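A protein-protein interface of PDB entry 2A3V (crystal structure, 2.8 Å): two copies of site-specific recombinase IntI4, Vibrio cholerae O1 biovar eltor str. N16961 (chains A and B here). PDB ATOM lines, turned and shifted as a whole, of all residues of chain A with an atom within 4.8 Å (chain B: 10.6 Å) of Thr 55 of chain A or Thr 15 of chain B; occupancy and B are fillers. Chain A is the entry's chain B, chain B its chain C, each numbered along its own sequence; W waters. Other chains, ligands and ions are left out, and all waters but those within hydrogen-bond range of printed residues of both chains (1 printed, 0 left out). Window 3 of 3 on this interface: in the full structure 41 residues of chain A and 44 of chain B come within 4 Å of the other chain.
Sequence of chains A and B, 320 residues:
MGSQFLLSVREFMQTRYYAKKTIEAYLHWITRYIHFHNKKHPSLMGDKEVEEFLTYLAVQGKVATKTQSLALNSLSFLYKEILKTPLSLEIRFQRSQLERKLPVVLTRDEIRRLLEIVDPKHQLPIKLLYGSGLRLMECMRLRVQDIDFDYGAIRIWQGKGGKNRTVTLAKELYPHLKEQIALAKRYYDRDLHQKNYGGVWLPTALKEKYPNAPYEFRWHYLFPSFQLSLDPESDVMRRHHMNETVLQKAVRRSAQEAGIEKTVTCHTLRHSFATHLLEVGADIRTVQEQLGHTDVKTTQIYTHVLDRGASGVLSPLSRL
Of the 17 printed residues of chain B, 4 touch a printed residue of chain A.
Hydrophobic or aromatic side chains of chain B within 4 Å of the printed part of chain A: Tyr 17.
Among the printed residues, 7 pairs touch across the chains.
Among the printed residues, Asp or Glu carboxylates within 4 Å of a Lys or Arg side-chain nitrogen of the other chain: Glu 51 of chain A with Arg 16 of chain B.
Thr 15 of chain B touches Ala 58 of chain A.
CA of Ala 58 of chain A touches OH of Tyr 17 of chain B, at 3.5 Å.
Gln 14 of chain B touches Val 59 of chain A.
Gln 68 of chain A touches Thr 15 of chain B (NE2 to O, 3.7 Å).
Gln 68 of chain A touches Tyr 17 of chain B (OE1 to CE1, 3.5 Å).
No position is printed for both chains.
OE2 of Glu 51 of chain A is in salt-bridge range of NH2 of Arg 16 of chain B, at 3.9 Å.
OG1 of Thr 15 of chain B sits at hydrogen-bond distance from OG1 of Thr 55 of chain A, 3.1 Å away.
Of chain A, only Thr 55, Ala 58 and Gln 68 come within 4 Å of Thr 15 of chain B.
No residue of chain B comes within 4 Å of Leu 54 of chain A.
Val 59 of chain A touches just one residue of chain B: Gln 14 (3.2 Å).
Printed residues of chain B within 4 Å of Ala 58 of chain A: Thr 15 and Tyr 17.
Of the printed residues of chain A, Tyr 17 of chain B touches Ala 58 (3.5 Å) and Gln 68 (3.5 Å).
Printed residues of chain A within 4 Å of Gln 14 of chain B: Val 59.
Printed residues of chain A within 4 Å of Arg 16 of chain B: Glu 51 (3.9 Å).
Of the printed residues of chain B, Gln 68 of chain A touches Thr 15 and Tyr 17.
The nearest printed residue of chain B that does not touch Gln 68 of chain A is Gln 14 of chain B (5.7 Å).
The backbone carbonyl oxygen (O) of Phe 12 of chain B is in hydrogen-bond range of the guanidinium group (NH1) of Arg 16 of chain B (2.9 Å).
The side-chain hydroxyl (OG1) of Thr 55 of chain A is in hydrogen-bond range of the backbone carbonyl oxygen (O) of Glu 51 of chain A (2.8 Å).
The backbone carbonyl oxygen (O) of Leu 54 of chain A is in hydrogen-bond range of the side-chain amide nitrogen (NE2) of Gln 68 of chain A.
The side-chain amide oxygen (OE1) of Gln 14 of chain B lies within hydrogen-bond range of the side-chain amino group (NZ) of Lys 20 of chain B (2.8 Å).
The backbone carbonyl oxygen (O) of Glu 11 of chain B sits at hydrogen-bond distance from the side-chain hydroxyl (OG1) of Thr 15 of chain B (3.1 Å).
The side-chain carboxylate (OE2) of Glu 11 of chain B is in hydrogen-bond range of the side-chain amide nitrogen (NE2) of Gln 14 of chain B (3.3 Å).
Water W1 lies within hydrogen-bond range of the side-chain amide oxygen (OE1) of Gln 68 of chain A and the backbone carbonyl oxygen (O) of Thr 15 of chain B.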
ATOM      1  N   GLU A  51      22.034   7.872  26.365  1.00  0.00           N
ATOM      2  CA  GLU A  51      20.629   7.543  26.565  1.00  0.00           C
ATOM      3  C   GLU A  51      19.770   7.957  25.365  1.00  0.00           C
ATOM      4  O   GLU A  51      18.834   7.252  24.987  1.00  0.00           O
ATOM      5  CB  GLU A  51      20.103   8.205  27.838  1.00  0.00           C
ATOM      6  CG  GLU A  51      18.755   7.655  28.284  1.00  0.00           C
ATOM      7  CD  GLU A  51      18.382   8.060  29.710  1.00  0.00           C
ATOM      8  OE1 GLU A  51      19.272   8.015  30.594  1.00  0.00           O
ATOM      9  OE2 GLU A  51      17.199   8.398  29.952  1.00  0.00           O
ATOM     10  N   GLU A  52      20.087   9.098  24.766  1.00  0.00           N
ATOM     11  CA  GLU A  52      19.340   9.561  23.606  1.00  0.00           C
ATOM     12  C   GLU A  52      19.525   8.578  22.463  1.00  0.00           C
ATOM     13  O   GLU A  52      18.604   8.342  21.691  1.00  0.00           O
ATOM     14  CB  GLU A  52      19.826  10.949  23.177  1.00  0.00           C
ATOM     15  CG  GLU A  52      19.515  12.074  24.166  1.00  0.00           C
ATOM     16  CD  GLU A  52      20.159  13.414  23.780  1.00  0.00           C
ATOM     17  OE1 GLU A  52      19.934  14.419  24.506  1.00  0.00           O
ATOM     18  OE2 GLU A  52      20.894  13.460  22.756  1.00  0.00           O
ATOM     19  N   PHE A  53      20.721   8.007  22.358  1.00  0.00           N
ATOM     20  CA  PHE A  53      21.016   7.040  21.305  1.00  0.00           C
ATOM     21  C   PHE A  53      20.271   5.727  21.553  1.00  0.00           C
ATOM     22  O   PHE A  53      19.635   5.165  20.651  1.00  0.00           O
ATOM     23  CB  PHE A  53      22.519   6.783  21.244  1.00  0.00           C
ATOM     24  CG  PHE A  53      22.917   5.762  20.222  1.00  0.00           C
ATOM     25  CD1 PHE A  53      22.513   5.889  18.898  1.00  0.00           C
ATOM     26  CD2 PHE A  53      23.697   4.677  20.584  1.00  0.00           C
ATOM     27  CE1 PHE A  53      22.881   4.947  17.947  1.00  0.00           C
ATOM     28  CE2 PHE A  53      24.070   3.732  19.647  1.00  0.00           C
ATOM     29  CZ  PHE A  53      23.661   3.866  18.323  1.00  0.00           C
ATOM     30  N   LEU A  54      20.369   5.242  22.786  1.00  0.00           N
ATOM     31  CA  LEU A  54      19.686   4.018  23.188  1.00  0.00           C
ATOM     32  C   LEU A  54      18.188   4.184  22.926  1.00  0.00           C
ATOM     33  O   LEU A  54      17.562   3.324  22.311  1.00  0.00           O
ATOM     34  CB  LEU A  54      19.949   3.739  24.677  1.00  0.00           C
ATOM     35  CG  LEU A  54      21.079   2.751  25.013  1.00  0.00           C
ATOM     36  CD1 LEU A  54      22.172   2.806  23.954  1.00  0.00           C
ATOM     37  CD2 LEU A  54      21.639   3.052  26.403  1.00  0.00           C
ATOM     38  N   THR A  55      17.622   5.301  23.378  1.00  0.00           N
ATOM     39  CA  THR A  55      16.209   5.563  23.167  1.00  0.00           C
ATOM     40  C   THR A  55      15.903   5.569  21.684  1.00  0.00           C
ATOM     41  O   THR A  55      14.841   5.131  21.254  1.00  0.00           O
ATOM     42  CB  THR A  55      15.797   6.917  23.714  1.00  0.00           C
ATOM     43  OG1 THR A  55      16.084   6.972  25.115  1.00  0.00           O
ATOM     44  CG2 THR A  55      14.309   7.140  23.485  1.00  0.00           C
ATOM     45  N   TYR A  56      16.839   6.084  20.903  1.00  0.00           N
ATOM     46  CA  TYR A  56      16.667   6.139  19.461  1.00  0.00           C
ATOM     47  C   TYR A  56      16.524   4.719  18.905  1.00  0.00           C
ATOM     48  O   TYR A  56      15.594   4.418  18.146  1.00  0.00           O
ATOM     49  CB  TYR A  56      17.870   6.852  18.843  1.00  0.00           C
ATOM     50  CG  TYR A  56      18.029   6.624  17.368  1.00  0.00           C
ATOM     51  CD1 TYR A  56      17.080   7.095  16.455  1.00  0.00           C
ATOM     52  CD2 TYR A  56      19.138   5.928  16.877  1.00  0.00           C
ATOM     53  CE1 TYR A  56      17.237   6.873  15.088  1.00  0.00           C
ATOM     54  CE2 TYR A  56      19.305   5.700  15.516  1.00  0.00           C
ATOM     55  CZ  TYR A  56      18.360   6.173  14.630  1.00  0.00           C
ATOM     56  OH  TYR A  56      18.558   5.949  13.285  1.00  0.00           O
ATOM     57  N   LEU A  57      17.443   3.847  19.306  1.00  0.00           N
ATOM     58  CA  LEU A  57      17.427   2.465  18.863  1.00  0.00           C
ATOM     59  C   LEU A  57      16.133   1.787  19.261  1.00  0.00           C
ATOM     60  O   LEU A  57      15.509   1.087  18.468  1.00  0.00           O
ATOM     61  CB  LEU A  57      18.606   1.722  19.477  1.00  0.00           C
ATOM     62  CG  LEU A  57      19.963   2.259  19.038  1.00  0.00           C
ATOM     63  CD1 LEU A  57      21.066   1.539  19.790  1.00  0.00           C
ATOM     64  CD2 LEU A  57      20.121   2.064  17.542  1.00  0.00           C
ATOM     65  N   ALA A  58      15.798   1.988  20.521  1.00  0.00           N
ATOM     66  CA  ALA A  58      14.609   1.396  21.080  1.00  0.00           C
ATOM     67  C   ALA A  58      13.398   1.851  20.342  1.00  0.00           C
ATOM     68  O   ALA A  58      12.588   1.049  19.853  1.00  0.00           O
ATOM     69  CB  ALA A  58      14.504   1.732  22.550  1.00  0.00           C
ATOM     70  N   VAL A  59      13.260   3.165  20.268  1.00  0.00           N
ATOM     71  CA  VAL A  59      12.089   3.702  19.588  1.00  0.00           C
ATOM     72  C   VAL A  59      12.401   3.818  18.100  1.00  0.00           C
ATOM     73  O   VAL A  59      13.382   3.240  17.661  1.00  0.00           O
ATOM     74  CB  VAL A  59      11.579   4.964  20.284  1.00  0.00           C
ATOM     75  CG1 VAL A  59      10.767   5.831  19.339  1.00  0.00           C
ATOM     76  CG2 VAL A  59      10.770   4.589  21.515  1.00  0.00           C
ATOM     77  N   GLN A  68      19.982  -3.580  22.026  1.00  0.00           N
ATOM     78  CA  GLN A  68      20.181  -2.268  22.610  1.00  0.00           C
ATOM     79  C   GLN A  68      21.104  -2.406  23.788  1.00  0.00           C
ATOM     80  O   GLN A  68      21.823  -1.497  24.175  1.00  0.00           O
ATOM     81  CB  GLN A  68      18.873  -1.694  23.094  1.00  0.00           C
ATOM     82  CG  GLN A  68      19.045  -0.316  23.668  1.00  0.00           C
ATOM     83  CD  GLN A  68      18.044  -0.056  24.738  1.00  0.00           C
ATOM     84  OE1 GLN A  68      17.990  -0.787  25.728  1.00  0.00           O
ATOM     85  NE2 GLN A  68      17.235   0.985  24.561  1.00  0.00           N
ATOM     86  N   LEU B   7       3.973  12.144  26.178  1.00  0.00           N
ATOM     87  CA  LEU B   7       4.828  11.562  25.159  1.00  0.00           C
ATOM     88  C   LEU B   7       6.182  11.205  25.747  1.00  0.00           C
ATOM     89  O   LEU B   7       6.806  10.241  25.323  1.00  0.00           O
ATOM     90  CB  LEU B   7       5.002  12.525  23.979  1.00  0.00           C
ATOM     91  CG  LEU B   7       5.779  12.043  22.732  1.00  0.00           C
ATOM     92  CD1 LEU B   7       7.286  12.008  23.003  1.00  0.00           C
ATOM     93  CD2 LEU B   7       5.268  10.665  22.304  1.00  0.00           C
ATOM     94  N   SER B   8       6.637  11.974  26.728  1.00  0.00           N
ATOM     95  CA  SER B   8       7.922  11.680  27.339  1.00  0.00           C
ATOM     96  C   SER B   8       7.788  10.415  28.182  1.00  0.00           C
ATOM     97  O   SER B   8       8.729   9.634  28.298  1.00  0.00           O
ATOM     98  CB  SER B   8       8.387  12.843  28.215  1.00  0.00           C
ATOM     99  OG  SER B   8       7.627  12.906  29.405  1.00  0.00           O
ATOM    100  N   VAL B   9       6.614  10.220  28.773  1.00  0.00           N
ATOM    101  CA  VAL B   9       6.356   9.037  29.590  1.00  0.00           C
ATOM    102  C   VAL B   9       6.355   7.808  28.692  1.00  0.00           C
ATOM    103  O   VAL B   9       6.891   6.771  29.051  1.00  0.00           O
ATOM    104  CB  VAL B   9       4.998   9.129  30.304  1.00  0.00           C
ATOM    105  CG1 VAL B   9       4.635   7.783  30.887  1.00  0.00           C
ATOM    106  CG2 VAL B   9       5.066  10.179  31.413  1.00  0.00           C
ATOM    107  N   ARG B  10       5.747   7.939  27.521  1.00  0.00           N
ATOM    108  CA  ARG B  10       5.701   6.849  26.571  1.00  0.00           C
ATOM    109  C   ARG B  10       7.120   6.503  26.119  1.00  0.00           C
ATOM    110  O   ARG B  10       7.450   5.339  25.954  1.00  0.00           O
ATOM    111  CB  ARG B  10       4.845   7.249  25.370  1.00  0.00           C
ATOM    112  CG  ARG B  10       4.750   6.192  24.279  1.00  0.00           C
ATOM    113  CD  ARG B  10       3.942   6.704  23.091  1.00  0.00           C
ATOM    114  NE  ARG B  10       2.623   7.186  23.505  1.00  0.00           N
ATOM    115  CZ  ARG B  10       1.579   6.404  23.759  1.00  0.00           C
ATOM    116  NH1 ARG B  10       1.689   5.089  23.639  1.00  0.00           N
ATOM    117  NH2 ARG B  10       0.423   6.941  24.133  1.00  0.00           N
ATOM    118  N   GLU B  11       7.965   7.512  25.925  1.00  0.00           N
ATOM    119  CA  GLU B  11       9.348   7.276  25.495  1.00  0.00           C
ATOM    120  C   GLU B  11      10.158   6.586  26.585  1.00  0.00           C
ATOM    121  O   GLU B  11      10.985   5.726  26.307  1.00  0.00           O
ATOM    122  CB  GLU B  11      10.052   8.599  25.155  1.00  0.00           C
ATOM    123  CG  GLU B  11       9.445   9.377  24.001  1.00  0.00           C
ATOM    124  CD  GLU B  11       9.675   8.710  22.655  1.00  0.00           C
ATOM    125  OE1 GLU B  11      10.847   8.692  22.189  1.00  0.00           O
ATOM    126  OE2 GLU B  11       8.684   8.201  22.067  1.00  0.00           O
ATOM    127  N   PHE B  12       9.938   6.997  27.825  1.00  0.00           N
ATOM    128  CA  PHE B  12      10.656   6.434  28.956  1.00  0.00           C
ATOM    129  C   PHE B  12      10.458   4.933  28.996  1.00  0.00           C
ATOM    130  O   PHE B  12      11.407   4.153  29.053  1.00  0.00           O
ATOM    131  CB  PHE B  12      10.101   7.026  30.229  1.00  0.00           C
ATOM    132  CG  PHE B  12      10.699   6.465  31.465  1.00  0.00           C
ATOM    133  CD1 PHE B  12      11.853   7.016  32.000  1.00  0.00           C
ATOM    134  CD2 PHE B  12      10.060   5.443  32.155  1.00  0.00           C
ATOM    135  CE1 PHE B  12      12.360   6.563  33.228  1.00  0.00           C
ATOM    136  CE2 PHE B  12      10.561   4.985  33.379  1.00  0.00           C
ATOM    137  CZ  PHE B  12      11.709   5.547  33.917  1.00  0.00           C
ATOM    138  N   MET B  13       9.185   4.563  28.976  1.00  0.00           N
ATOM    139  CA  MET B  13       8.754   3.190  29.013  1.00  0.00           C
ATOM    140  C   MET B  13       9.237   2.405  27.803  1.00  0.00           C
ATOM    141  O   MET B  13       9.686   1.279  27.952  1.00  0.00           O
ATOM    142  CB  MET B  13       7.227   3.136  29.123  1.00  0.00           C
ATOM    143  CG  MET B  13       6.702   3.644  30.466  1.00  0.00           C
ATOM    144  SD  MET B  13       4.911   3.594  30.610  1.00  0.00           S
ATOM    145  CE  MET B  13       4.644   1.915  31.067  1.00  0.00           C
ATOM    146  N   GLN B  14       9.169   2.972  26.607  1.00  0.00           N
ATOM    147  CA  GLN B  14       9.637   2.216  25.456  1.00  0.00           C
ATOM    148  C   GLN B  14      11.124   1.884  25.553  1.00  0.00           C
ATOM    149  O   GLN B  14      11.546   0.825  25.089  1.00  0.00           O
ATOM    150  CB  GLN B  14       9.385   2.971  24.157  1.00  0.00           C
ATOM    151  CG  GLN B  14       7.927   3.253  23.895  1.00  0.00           C
ATOM    152  CD  GLN B  14       7.691   3.879  22.537  1.00  0.00           C
ATOM    153  OE1 GLN B  14       7.834   3.218  21.505  1.00  0.00           O
ATOM    154  NE2 GLN B  14       7.342   5.167  22.525  1.00  0.00           N
ATOM    155  N   THR B  15      11.920   2.764  26.155  1.00  0.00           N
ATOM    156  CA  THR B  15      13.355   2.517  26.262  1.00  0.00           C
ATOM    157  C   THR B  15      13.636   1.405  27.246  1.00  0.00           C
ATOM    158  O   THR B  15      14.515   0.569  27.022  1.00  0.00           O
ATOM    159  CB  THR B  15      14.114   3.767  26.718  1.00  0.00           C
ATOM    160  OG1 THR B  15      13.898   4.812  25.770  1.00  0.00           O
ATOM    161  CG2 THR B  15      15.605   3.486  26.795  1.00  0.00           C
ATOM    162  N   ARG B  16      12.897   1.420  28.350  1.00  0.00           N
ATOM    163  CA  ARG B  16      13.017   0.409  29.394  1.00  0.00           C
ATOM    164  C   ARG B  16      12.319  -0.869  28.894  1.00  0.00           C
ATOM    165  O   ARG B  16      12.071  -1.795  29.656  1.00  0.00           O
ATOM    166  CB  ARG B  16      12.309   0.891  30.662  1.00  0.00           C
ATOM    167  CG  ARG B  16      12.644   2.329  31.096  1.00  0.00           C
ATOM    168  CD  ARG B  16      14.056   2.405  31.609  1.00  0.00           C
ATOM    169  NE  ARG B  16      14.447   3.723  32.109  1.00  0.00           N
ATOM    170  CZ  ARG B  16      14.434   4.844  31.391  1.00  0.00           C
ATOM    171  NH1 ARG B  16      14.025   4.838  30.122  1.00  0.00           N
ATOM    172  NH2 ARG B  16      14.892   5.965  31.930  1.00  0.00           N
ATOM    173  N   TYR B  17      11.979  -0.901  27.615  1.00  0.00           N
ATOM    174  CA  TYR B  17      11.313  -2.046  27.024  1.00  0.00           C
ATOM    175  C   TYR B  17      10.100  -2.616  27.749  1.00  0.00           C
ATOM    176  O   TYR B  17       9.963  -3.827  27.860  1.00  0.00           O
ATOM    177  CB  TYR B  17      12.320  -3.172  26.749  1.00  0.00           C
ATOM    178  CG  TYR B  17      13.150  -2.934  25.506  1.00  0.00           C
ATOM    179  CD1 TYR B  17      14.257  -2.085  25.524  1.00  0.00           C
ATOM    180  CD2 TYR B  17      12.764  -3.472  24.290  1.00  0.00           C
ATOM    181  CE1 TYR B  17      14.950  -1.775  24.362  1.00  0.00           C
ATOM    182  CE2 TYR B  17      13.444  -3.164  23.120  1.00  0.00           C
ATOM    183  CZ  TYR B  17      14.535  -2.311  23.160  1.00  0.00           C
ATOM    184  OH  TYR B  17      15.182  -1.968  21.991  1.00  0.00           O
ATOM    185  N   TYR B  18       9.208  -1.763  28.238  1.00  0.00           N
ATOM    186  CA  TYR B  18       7.988  -2.265  28.870  1.00  0.00           C
ATOM    187  C   TYR B  18       7.154  -2.820  27.718  1.00  0.00           C
ATOM    188  O   TYR B  18       7.330  -2.405  26.578  1.00  0.00           O
ATOM    189  CB  TYR B  18       7.206  -1.133  29.543  1.00  0.00           C
ATOM    190  CG  TYR B  18       7.682  -0.802  30.927  1.00  0.00           C
ATOM    191  CD1 TYR B  18       8.787   0.001  31.130  1.00  0.00           C
ATOM    192  CD2 TYR B  18       7.048  -1.345  32.038  1.00  0.00           C
ATOM    193  CE1 TYR B  18       9.257   0.255  32.406  1.00  0.00           C
ATOM    194  CE2 TYR B  18       7.506  -1.099  33.321  1.00  0.00           C
ATOM    195  CZ  TYR B  18       8.614  -0.300  33.502  1.00  0.00           C
ATOM    196  OH  TYR B  18       9.083  -0.081  34.785  1.00  0.00           O
ATOM    197  N   ALA B  19       6.248  -3.746  27.994  1.00  0.00           N
ATOM    198  CA  ALA B  19       5.422  -4.306  26.931  1.00  0.00           C
ATOM    199  C   ALA B  19       4.599  -3.191  26.283  1.00  0.00           C
ATOM    200  O   ALA B  19       4.372  -2.155  26.905  1.00  0.00           O
ATOM    201  CB  ALA B  19       4.506  -5.364  27.510  1.00  0.00           C
ATOM    202  N   LYS B  20       4.151  -3.377  25.044  1.00  0.00           N
ATOM    203  CA  LYS B  20       3.342  -2.333  24.415  1.00  0.00           C
ATOM    204  C   LYS B  20       2.037  -2.153  25.170  1.00  0.00           C
ATOM    205  O   LYS B  20       1.677  -1.036  25.541  1.00  0.00           O
ATOM    206  CB  LYS B  20       3.025  -2.665  22.953  1.00  0.00           C
ATOM    207  CG  LYS B  20       4.154  -2.340  21.990  1.00  0.00           C
ATOM    208  CD  LYS B  20       4.584  -0.872  22.152  1.00  0.00           C
ATOM    209  CE  LYS B  20       5.953  -0.574  21.532  1.00  0.00           C
ATOM    210  NZ  LYS B  20       6.357   0.836  21.834  1.00  0.00           N
ATOM    211  N   ILE B  23       2.292  -0.201  28.242  1.00  0.00           N
ATOM    212  CA  ILE B  23       2.388   1.230  28.028  1.00  0.00           C
ATOM    213  C   ILE B  23       0.998   1.822  27.802  1.00  0.00           C
ATOM    214  O   ILE B  23       0.648   2.830  28.405  1.00  0.00           O
ATOM    215  CB  ILE B  23       3.283   1.552  26.830  1.00  0.00           C
ATOM    216  CG1 ILE B  23       4.715   1.092  27.130  1.00  0.00           C
ATOM    217  CG2 ILE B  23       3.235   3.046  26.539  1.00  0.00           C
ATOM    218  CD1 ILE B  23       5.668   1.229  25.964  1.00  0.00           C
ATOM    219  N   PHE B  77       3.329   4.027  39.302  1.00  0.00           N
ATOM    220  CA  PHE B  77       4.441   4.001  38.361  1.00  0.00           C
ATOM    221  C   PHE B  77       4.873   5.434  38.066  1.00  0.00           C
ATOM    222  O   PHE B  77       6.052   5.778  38.183  1.00  0.00           O
ATOM    223  CB  PHE B  77       4.018   3.334  37.055  1.00  0.00           C
ATOM    224  CG  PHE B  77       5.017   3.499  35.932  1.00  0.00           C
ATOM    225  CD1 PHE B  77       6.248   2.847  35.969  1.00  0.00           C
ATOM    226  CD2 PHE B  77       4.710   4.290  34.824  1.00  0.00           C
ATOM    227  CE1 PHE B  77       7.155   2.978  34.916  1.00  0.00           C
ATOM    228  CE2 PHE B  77       5.611   4.429  33.764  1.00  0.00           C
ATOM    229  CZ  PHE B  77       6.832   3.772  33.810  1.00  0.00           C
ATOM    230  N   ILE B  82       8.752   8.061  36.836  1.00  0.00           N
ATOM    231  CA  ILE B  82       8.805   9.340  36.132  1.00  0.00           C
ATOM    232  C   ILE B  82       9.244  10.452  37.089  1.00  0.00           C
ATOM    233  O   ILE B  82      10.404  10.853  37.077  1.00  0.00           O
ATOM    234  CB  ILE B  82       7.445   9.700  35.535  1.00  0.00           C
ATOM    235  CG1 ILE B  82       6.901   8.516  34.737  1.00  0.00           C
ATOM    236  CG2 ILE B  82       7.593  10.894  34.610  1.00  0.00           C
ATOM    237  CD1 ILE B  82       7.805   8.082  33.621  1.00  0.00           C
HETATM  238  O   HOH W   1      17.122  -0.551  28.604  1.00  0.00           O
